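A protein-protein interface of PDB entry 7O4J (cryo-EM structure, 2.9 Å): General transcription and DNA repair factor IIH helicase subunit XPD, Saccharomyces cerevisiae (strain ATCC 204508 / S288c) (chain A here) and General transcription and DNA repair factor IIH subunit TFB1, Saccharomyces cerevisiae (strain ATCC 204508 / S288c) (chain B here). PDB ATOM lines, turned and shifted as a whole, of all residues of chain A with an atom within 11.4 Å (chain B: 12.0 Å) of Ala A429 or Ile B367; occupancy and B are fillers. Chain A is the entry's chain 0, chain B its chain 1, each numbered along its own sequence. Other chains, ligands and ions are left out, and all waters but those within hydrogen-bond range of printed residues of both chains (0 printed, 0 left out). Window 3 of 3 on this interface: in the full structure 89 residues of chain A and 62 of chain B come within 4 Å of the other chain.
ND2 of Asn A427 lies within hydrogen-bond range of O of Val B365, at 3.4 Å.
The backbone NH (N) of Ala A429 sits at hydrogen-bond distance from the backbone carbonyl oxygen (O) of Ile B367, 3.0 Å away.
Among the printed residues, pairs that only touch across the chains: Ile A425 with Phe B359 (3.9 Å), Asn A427 with Asp B366 (3.6 Å), Asn A427 with Ile B367 (2.9 Å) and Ala A428 with Ile B367 (3.6 Å).
Glu A426 touches none of the printed residues of chain B.
Asn A427 touches just these residues of chain B: Val B365, Asp B366 and Ile B367.
Ala A428 touches one residue of chain B.
Ala A429 touches just one residue of chain B: Ile B367 (3.0 Å).
No residue of chain B comes within 4 Å of Val A430.
No residue of chain B comes within 4 Å of Pro A431.
Of the printed residues of chain A, Phe B359 touches Ile A425.
Of the printed residues of chain A, Val B365 touches Asn A427.
Of chain A, only Asn A427 comes within 4 Å of Asp B366.
Of chain A, only Asn A427, Ala A428 and Ala A429 come within 4 Å of Ile B367.
No residue of chain A comes within 4 Å of Asn B368.
Ser B371 touches none of the printed residues of chain A.
The nearest printed residue of chain B that does not touch Ile A425 is Val B365 (4.8 Å).
Of the 12 printed residues of chain B, 4 touch a printed residue of chain A.
Printed residues of chain B that touch a printed residue of chain A: Phe B359, Val B365, Asp B366 and Ile B367.
Hydrophobic or aromatic side chains of chain A that line the printed part of chain B: Ile A425 and Ala A429.
Among the printed residues, no Asp or Glu carboxylate lies within 4 Å of a Lys or Arg side-chain nitrogen of the other chain.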
ATOM      1  N   PRO A 422       5.039 -30.663 -12.290  1.00  0.00           N
ATOM      2  CA  PRO A 422       5.670 -31.625 -11.374  1.00  0.00           C
ATOM      3  C   PRO A 422       6.562 -30.978 -10.330  1.00  0.00           C
ATOM      4  O   PRO A 422       6.984 -31.669  -9.394  1.00  0.00           O
ATOM      5  CB  PRO A 422       6.480 -32.523 -12.314  1.00  0.00           C
ATOM      6  CG  PRO A 422       6.782 -31.664 -13.485  1.00  0.00           C
ATOM      7  CD  PRO A 422       5.617 -30.732 -13.644  1.00  0.00           C
ATOM      8  N   TYR A 423       6.861 -29.685 -10.456  1.00  0.00           N
ATOM      9  CA  TYR A 423       7.756 -28.990  -9.530  1.00  0.00           C
ATOM     10  C   TYR A 423       7.134 -27.643  -9.178  1.00  0.00           C
ATOM     11  O   TYR A 423       7.230 -26.691  -9.958  1.00  0.00           O
ATOM     12  CB  TYR A 423       9.142 -28.801 -10.135  1.00  0.00           C
ATOM     13  CG  TYR A 423       9.913 -30.079 -10.357  1.00  0.00           C
ATOM     14  CD1 TYR A 423      10.757 -30.581  -9.376  1.00  0.00           C
ATOM     15  CD2 TYR A 423       9.810 -30.778 -11.552  1.00  0.00           C
ATOM     16  CE1 TYR A 423      11.470 -31.746  -9.575  1.00  0.00           C
ATOM     17  CE2 TYR A 423      10.518 -31.944 -11.761  1.00  0.00           C
ATOM     18  CZ  TYR A 423      11.348 -32.423 -10.770  1.00  0.00           C
ATOM     19  OH  TYR A 423      12.056 -33.585 -10.973  1.00  0.00           O
ATOM     20  N   GLU A 424       6.499 -27.564  -8.008  1.00  0.00           N
ATOM     21  CA  GLU A 424       6.123 -26.259  -7.474  1.00  0.00           C
ATOM     22  C   GLU A 424       7.365 -25.428  -7.189  1.00  0.00           C
ATOM     23  O   GLU A 424       7.410 -24.228  -7.482  1.00  0.00           O
ATOM     24  CB  GLU A 424       5.282 -26.429  -6.209  1.00  0.00           C
ATOM     25  CG  GLU A 424       4.720 -25.122  -5.667  1.00  0.00           C
ATOM     26  CD  GLU A 424       4.038 -25.292  -4.325  1.00  0.00           C
ATOM     27  OE1 GLU A 424       3.855 -24.279  -3.617  1.00  0.00           O
ATOM     28  OE2 GLU A 424       3.685 -26.438  -3.977  1.00  0.00           O
ATOM     29  N   ILE A 425       8.387 -26.057  -6.615  1.00  0.00           N
ATOM     30  CA  ILE A 425       9.692 -25.447  -6.402  1.00  0.00           C
ATOM     31  C   ILE A 425      10.698 -26.260  -7.205  1.00  0.00           C
ATOM     32  O   ILE A 425      10.968 -27.423  -6.880  1.00  0.00           O
ATOM     33  CB  ILE A 425      10.071 -25.409  -4.915  1.00  0.00           C
ATOM     34  CG1 ILE A 425       9.010 -24.659  -4.104  1.00  0.00           C
ATOM     35  CG2 ILE A 425      11.441 -24.773  -4.731  1.00  0.00           C
ATOM     36  CD1 ILE A 425       8.864 -23.194  -4.470  1.00  0.00           C
ATOM     37  N   GLU A 426      11.255 -25.654  -8.254  1.00  0.00           N
ATOM     38  CA  GLU A 426      12.242 -26.354  -9.070  1.00  0.00           C
ATOM     39  C   GLU A 426      13.491 -26.707  -8.274  1.00  0.00           C
ATOM     40  O   GLU A 426      14.214 -27.634  -8.654  1.00  0.00           O
ATOM     41  CB  GLU A 426      12.620 -25.503 -10.283  1.00  0.00           C
ATOM     42  CG  GLU A 426      13.279 -24.179  -9.932  1.00  0.00           C
ATOM     43  CD  GLU A 426      13.517 -23.306 -11.149  1.00  0.00           C
ATOM     44  OE1 GLU A 426      13.494 -23.839 -12.278  1.00  0.00           O
ATOM     45  OE2 GLU A 426      13.726 -22.088 -10.974  1.00  0.00           O
ATOM     46  N   ASN A 427      13.757 -25.991  -7.186  1.00  0.00           N
ATOM     47  CA  ASN A 427      14.923 -26.251  -6.344  1.00  0.00           C
ATOM     48  C   ASN A 427      14.509 -27.130  -5.164  1.00  0.00           C
ATOM     49  O   ASN A 427      14.412 -26.694  -4.017  1.00  0.00           O
ATOM     50  CB  ASN A 427      15.536 -24.932  -5.879  1.00  0.00           C
ATOM     51  CG  ASN A 427      16.681 -25.130  -4.909  1.00  0.00           C
ATOM     52  OD1 ASN A 427      17.753 -25.603  -5.285  1.00  0.00           O
ATOM     53  ND2 ASN A 427      16.462 -24.766  -3.651  1.00  0.00           N
ATOM     54  N   ALA A 428      14.258 -28.400  -5.476  1.00  0.00           N
ATOM     55  CA  ALA A 428      13.801 -29.356  -4.477  1.00  0.00           C
ATOM     56  C   ALA A 428      14.365 -30.732  -4.796  1.00  0.00           C
ATOM     57  O   ALA A 428      14.469 -31.112  -5.965  1.00  0.00           O
ATOM     58  CB  ALA A 428      12.270 -29.415  -4.423  1.00  0.00           C
ATOM     59  N   ALA A 429      14.727 -31.472  -3.745  1.00  0.00           N
ATOM     60  CA  ALA A 429      15.245 -32.822  -3.936  1.00  0.00           C
ATOM     61  C   ALA A 429      14.187 -33.743  -4.526  1.00  0.00           C
ATOM     62  O   ALA A 429      14.479 -34.536  -5.429  1.00  0.00           O
ATOM     63  CB  ALA A 429      15.753 -33.381  -2.608  1.00  0.00           C
ATOM     64  N   VAL A 430      12.956 -33.653  -4.032  1.00  0.00           N
ATOM     65  CA  VAL A 430      11.862 -34.525  -4.443  1.00  0.00           C
ATOM     66  C   VAL A 430      10.804 -33.660  -5.112  1.00  0.00           C
ATOM     67  O   VAL A 430      10.462 -32.602  -4.583  1.00  0.00           O
ATOM     68  CB  VAL A 430      11.251 -35.298  -3.260  1.00  0.00           C
ATOM     69  CG1 VAL A 430      12.322 -36.111  -2.549  1.00  0.00           C
ATOM     70  CG2 VAL A 430      10.568 -34.344  -2.288  1.00  0.00           C
ATOM     71  N   PRO A 431      10.267 -34.054  -6.269  1.00  0.00           N
ATOM     72  CA  PRO A 431       9.215 -33.248  -6.894  1.00  0.00           C
ATOM     73  C   PRO A 431       7.995 -33.126  -5.994  1.00  0.00           C
ATOM     74  O   PRO A 431       7.642 -34.049  -5.258  1.00  0.00           O
ATOM     75  CB  PRO A 431       8.885 -34.018  -8.178  1.00  0.00           C
ATOM     76  CG  PRO A 431      10.065 -34.880  -8.436  1.00  0.00           C
ATOM     77  CD  PRO A 431      10.660 -35.202  -7.105  1.00  0.00           C
ATOM     78  N   ASN A 432       7.352 -31.963  -6.062  1.00  0.00           N
ATOM     79  CA  ASN A 432       6.118 -31.695  -5.325  1.00  0.00           C
ATOM     80  C   ASN A 432       5.073 -31.206  -6.320  1.00  0.00           C
ATOM     81  O   ASN A 432       4.936 -29.988  -6.532  1.00  0.00           O
ATOM     82  CB  ASN A 432       6.346 -30.672  -4.219  1.00  0.00           C
ATOM     83  CG  ASN A 432       5.326 -30.786  -3.101  1.00  0.00           C
ATOM     84  OD1 ASN A 432       4.592 -31.770  -3.011  1.00  0.00           O
ATOM     85  ND2 ASN A 432       5.280 -29.777  -2.239  1.00  0.00           N
ATOM     86  N   PRO A 433       4.326 -32.109  -6.952  1.00  0.00           N
ATOM     87  CA  PRO A 433       3.386 -31.682  -7.993  1.00  0.00           C
ATOM     88  C   PRO A 433       2.322 -30.741  -7.453  1.00  0.00           C
ATOM     89  O   PRO A 433       1.870 -30.858  -6.311  1.00  0.00           O
ATOM     90  CB  PRO A 433       2.765 -32.998  -8.481  1.00  0.00           C
ATOM     91  CG  PRO A 433       3.652 -34.081  -7.964  1.00  0.00           C
ATOM     92  CD  PRO A 433       4.259 -33.559  -6.710  1.00  0.00           C
ATOM     93  N   ARG A 513      21.875 -11.418  -9.344  1.00  0.00           N
ATOM     94  CA  ARG A 513      21.693 -10.893  -7.995  1.00  0.00           C
ATOM     95  C   ARG A 513      22.945 -11.094  -7.150  1.00  0.00           C
ATOM     96  O   ARG A 513      23.324 -10.210  -6.373  1.00  0.00           O
ATOM     97  CB  ARG A 513      20.481 -11.549  -7.333  1.00  0.00           C
ATOM     98  CG  ARG A 513      20.556 -13.063  -7.227  1.00  0.00           C
ATOM     99  CD  ARG A 513      19.275 -13.631  -6.639  1.00  0.00           C
ATOM    100  NE  ARG A 513      19.147 -15.068  -6.869  1.00  0.00           N
ATOM    101  CZ  ARG A 513      19.593 -16.011  -6.042  1.00  0.00           C
ATOM    102  NH1 ARG A 513      20.209 -15.686  -4.914  1.00  0.00           N
ATOM    103  NH2 ARG A 513      19.422 -17.289  -6.350  1.00  0.00           N
ATOM    104  N   PHE B 359       8.497 -18.615  -6.097  1.00  0.00           N
ATOM    105  CA  PHE B 359       9.551 -18.747  -5.098  1.00  0.00           C
ATOM    106  C   PHE B 359      10.294 -17.439  -4.865  1.00  0.00           C
ATOM    107  O   PHE B 359      10.954 -17.293  -3.831  1.00  0.00           O
ATOM    108  CB  PHE B 359      10.536 -19.839  -5.516  1.00  0.00           C
ATOM    109  CG  PHE B 359      11.571 -19.378  -6.500  1.00  0.00           C
ATOM    110  CD1 PHE B 359      11.207 -19.000  -7.779  1.00  0.00           C
ATOM    111  CD2 PHE B 359      12.908 -19.325  -6.146  1.00  0.00           C
ATOM    112  CE1 PHE B 359      12.156 -18.577  -8.687  1.00  0.00           C
ATOM    113  CE2 PHE B 359      13.861 -18.902  -7.050  1.00  0.00           C
ATOM    114  CZ  PHE B 359      13.485 -18.527  -8.322  1.00  0.00           C
ATOM    115  N   PRO B 363      10.256 -16.814   1.330  1.00  0.00           N
ATOM    116  CA  PRO B 363      11.588 -16.964   1.924  1.00  0.00           C
ATOM    117  C   PRO B 363      12.368 -18.089   1.263  1.00  0.00           C
ATOM    118  O   PRO B 363      11.812 -19.117   0.870  1.00  0.00           O
ATOM    119  CB  PRO B 363      11.293 -17.280   3.395  1.00  0.00           C
ATOM    120  CG  PRO B 363       9.907 -16.794   3.626  1.00  0.00           C
ATOM    121  CD  PRO B 363       9.187 -16.976   2.330  1.00  0.00           C
ATOM    122  N   GLY B 364      13.676 -17.879   1.143  1.00  0.00           N
ATOM    123  CA  GLY B 364      14.515 -18.860   0.488  1.00  0.00           C
ATOM    124  C   GLY B 364      14.567 -20.171   1.249  1.00  0.00           C
ATOM    125  O   GLY B 364      14.481 -20.215   2.476  1.00  0.00           O
ATOM    126  N   VAL B 365      14.710 -21.261   0.494  1.00  0.00           N
ATOM    127  CA  VAL B 365      14.833 -22.601   1.047  1.00  0.00           C
ATOM    128  C   VAL B 365      15.938 -23.333   0.295  1.00  0.00           C
ATOM    129  O   VAL B 365      16.360 -22.927  -0.787  1.00  0.00           O
ATOM    130  CB  VAL B 365      13.510 -23.393   0.971  1.00  0.00           C
ATOM    131  CG1 VAL B 365      12.530 -22.890   2.019  1.00  0.00           C
ATOM    132  CG2 VAL B 365      12.908 -23.294  -0.422  1.00  0.00           C
ATOM    133  N   ASP B 366      16.403 -24.427   0.890  1.00  0.00           N
ATOM    134  CA  ASP B 366      17.468 -25.236   0.322  1.00  0.00           C
ATOM    135  C   ASP B 366      16.873 -26.426  -0.429  1.00  0.00           C
ATOM    136  O   ASP B 366      15.657 -26.557  -0.583  1.00  0.00           O
ATOM    137  CB  ASP B 366      18.428 -25.696   1.422  1.00  0.00           C
ATOM    138  CG  ASP B 366      19.291 -24.568   1.953  1.00  0.00           C
ATOM    139  OD1 ASP B 366      19.348 -23.502   1.303  1.00  0.00           O
ATOM    140  OD2 ASP B 366      19.915 -24.748   3.019  1.00  0.00           O
ATOM    141  N   ILE B 367      17.756 -27.308  -0.904  1.00  0.00           N
ATOM    142  CA  ILE B 367      17.308 -28.478  -1.655  1.00  0.00           C
ATOM    143  C   ILE B 367      16.413 -29.356  -0.791  1.00  0.00           C
ATOM    144  O   ILE B 367      15.377 -29.853  -1.249  1.00  0.00           O
ATOM    145  CB  ILE B 367      18.521 -29.264  -2.189  1.00  0.00           C
ATOM    146  CG1 ILE B 367      19.390 -28.380  -3.089  1.00  0.00           C
ATOM    147  CG2 ILE B 367      18.062 -30.504  -2.937  1.00  0.00           C
ATOM    148  CD1 ILE B 367      18.818 -28.162  -4.474  1.00  0.00           C
ATOM    149  N   ASN B 368      16.793 -29.560   0.471  1.00  0.00           N
ATOM    150  CA  ASN B 368      16.016 -30.401   1.372  1.00  0.00           C
ATOM    151  C   ASN B 368      14.684 -29.778   1.771  1.00  0.00           C
ATOM    152  O   ASN B 368      13.840 -30.478   2.338  1.00  0.00           O
ATOM    153  CB  ASN B 368      16.831 -30.713   2.628  1.00  0.00           C
ATOM    154  CG  ASN B 368      18.234 -31.188   2.308  1.00  0.00           C
ATOM    155  OD1 ASN B 368      18.501 -31.674   1.208  1.00  0.00           O
ATOM    156  ND2 ASN B 368      19.141 -31.050   3.267  1.00  0.00           N
ATOM    157  N   GLY B 369      14.475 -28.491   1.493  1.00  0.00           N
ATOM    158  CA  GLY B 369      13.212 -27.835   1.750  1.00  0.00           C
ATOM    159  C   GLY B 369      13.165 -27.002   3.013  1.00  0.00           C
ATOM    160  O   GLY B 369      12.184 -26.274   3.213  1.00  0.00           O
ATOM    161  N   ASN B 370      14.182 -27.079   3.865  1.00  0.00           N
ATOM    162  CA  ASN B 370      14.197 -26.312   5.100  1.00  0.00           C
ATOM    163  C   ASN B 370      14.750 -24.910   4.853  1.00  0.00           C
ATOM    164  O   ASN B 370      15.348 -24.618   3.814  1.00  0.00           O
ATOM    165  CB  ASN B 370      15.013 -27.033   6.175  1.00  0.00           C
ATOM    166  CG  ASN B 370      16.384 -27.453   5.686  1.00  0.00           C
ATOM    167  OD1 ASN B 370      16.566 -27.775   4.511  1.00  0.00           O
ATOM    168  ND2 ASN B 370      17.358 -27.458   6.589  1.00  0.00           N
ATOM    169  N   SER B 371      14.543 -24.034   5.833  1.00  0.00           N
ATOM    170  CA  SER B 371      14.907 -22.634   5.680  1.00  0.00           C
ATOM    171  C   SER B 371      16.416 -22.475   5.535  1.00  0.00           C
ATOM    172  O   SER B 371      17.205 -23.189   6.160  1.00  0.00           O
ATOM    173  CB  SER B 371      14.412 -21.825   6.880  1.00  0.00           C
ATOM    174  OG  SER B 371      14.728 -20.452   6.736  1.00  0.00           O
ATOM    175  N   ASP B 372      16.814 -21.517   4.694  1.00  0.00           N
ATOM    176  CA  ASP B 372      18.227 -21.209   4.511  1.00  0.00           C
ATOM    177  C   ASP B 372      18.805 -20.402   5.667  1.00  0.00           C
ATOM    178  O   ASP B 372      20.028 -20.400   5.850  1.00  0.00           O
ATOM    179  CB  ASP B 372      18.431 -20.447   3.200  1.00  0.00           C
ATOM    180  CG  ASP B 372      17.698 -19.123   3.176  1.00  0.00           C
ATOM    181  OD1 ASP B 372      16.845 -18.900   4.061  1.00  0.00           O
ATOM    182  OD2 ASP B 372      17.974 -18.306   2.274  1.00  0.00           O
ATOM    183  N   GLY B 373      17.966 -19.721   6.440  1.00  0.00           N
ATOM    184  CA  GLY B 373      18.407 -19.028   7.632  1.00  0.00           C
ATOM    185  C   GLY B 373      18.608 -17.535   7.501  1.00  0.00           C
ATOM    186  O   GLY B 373      18.952 -16.890   8.498  1.00  0.00           O
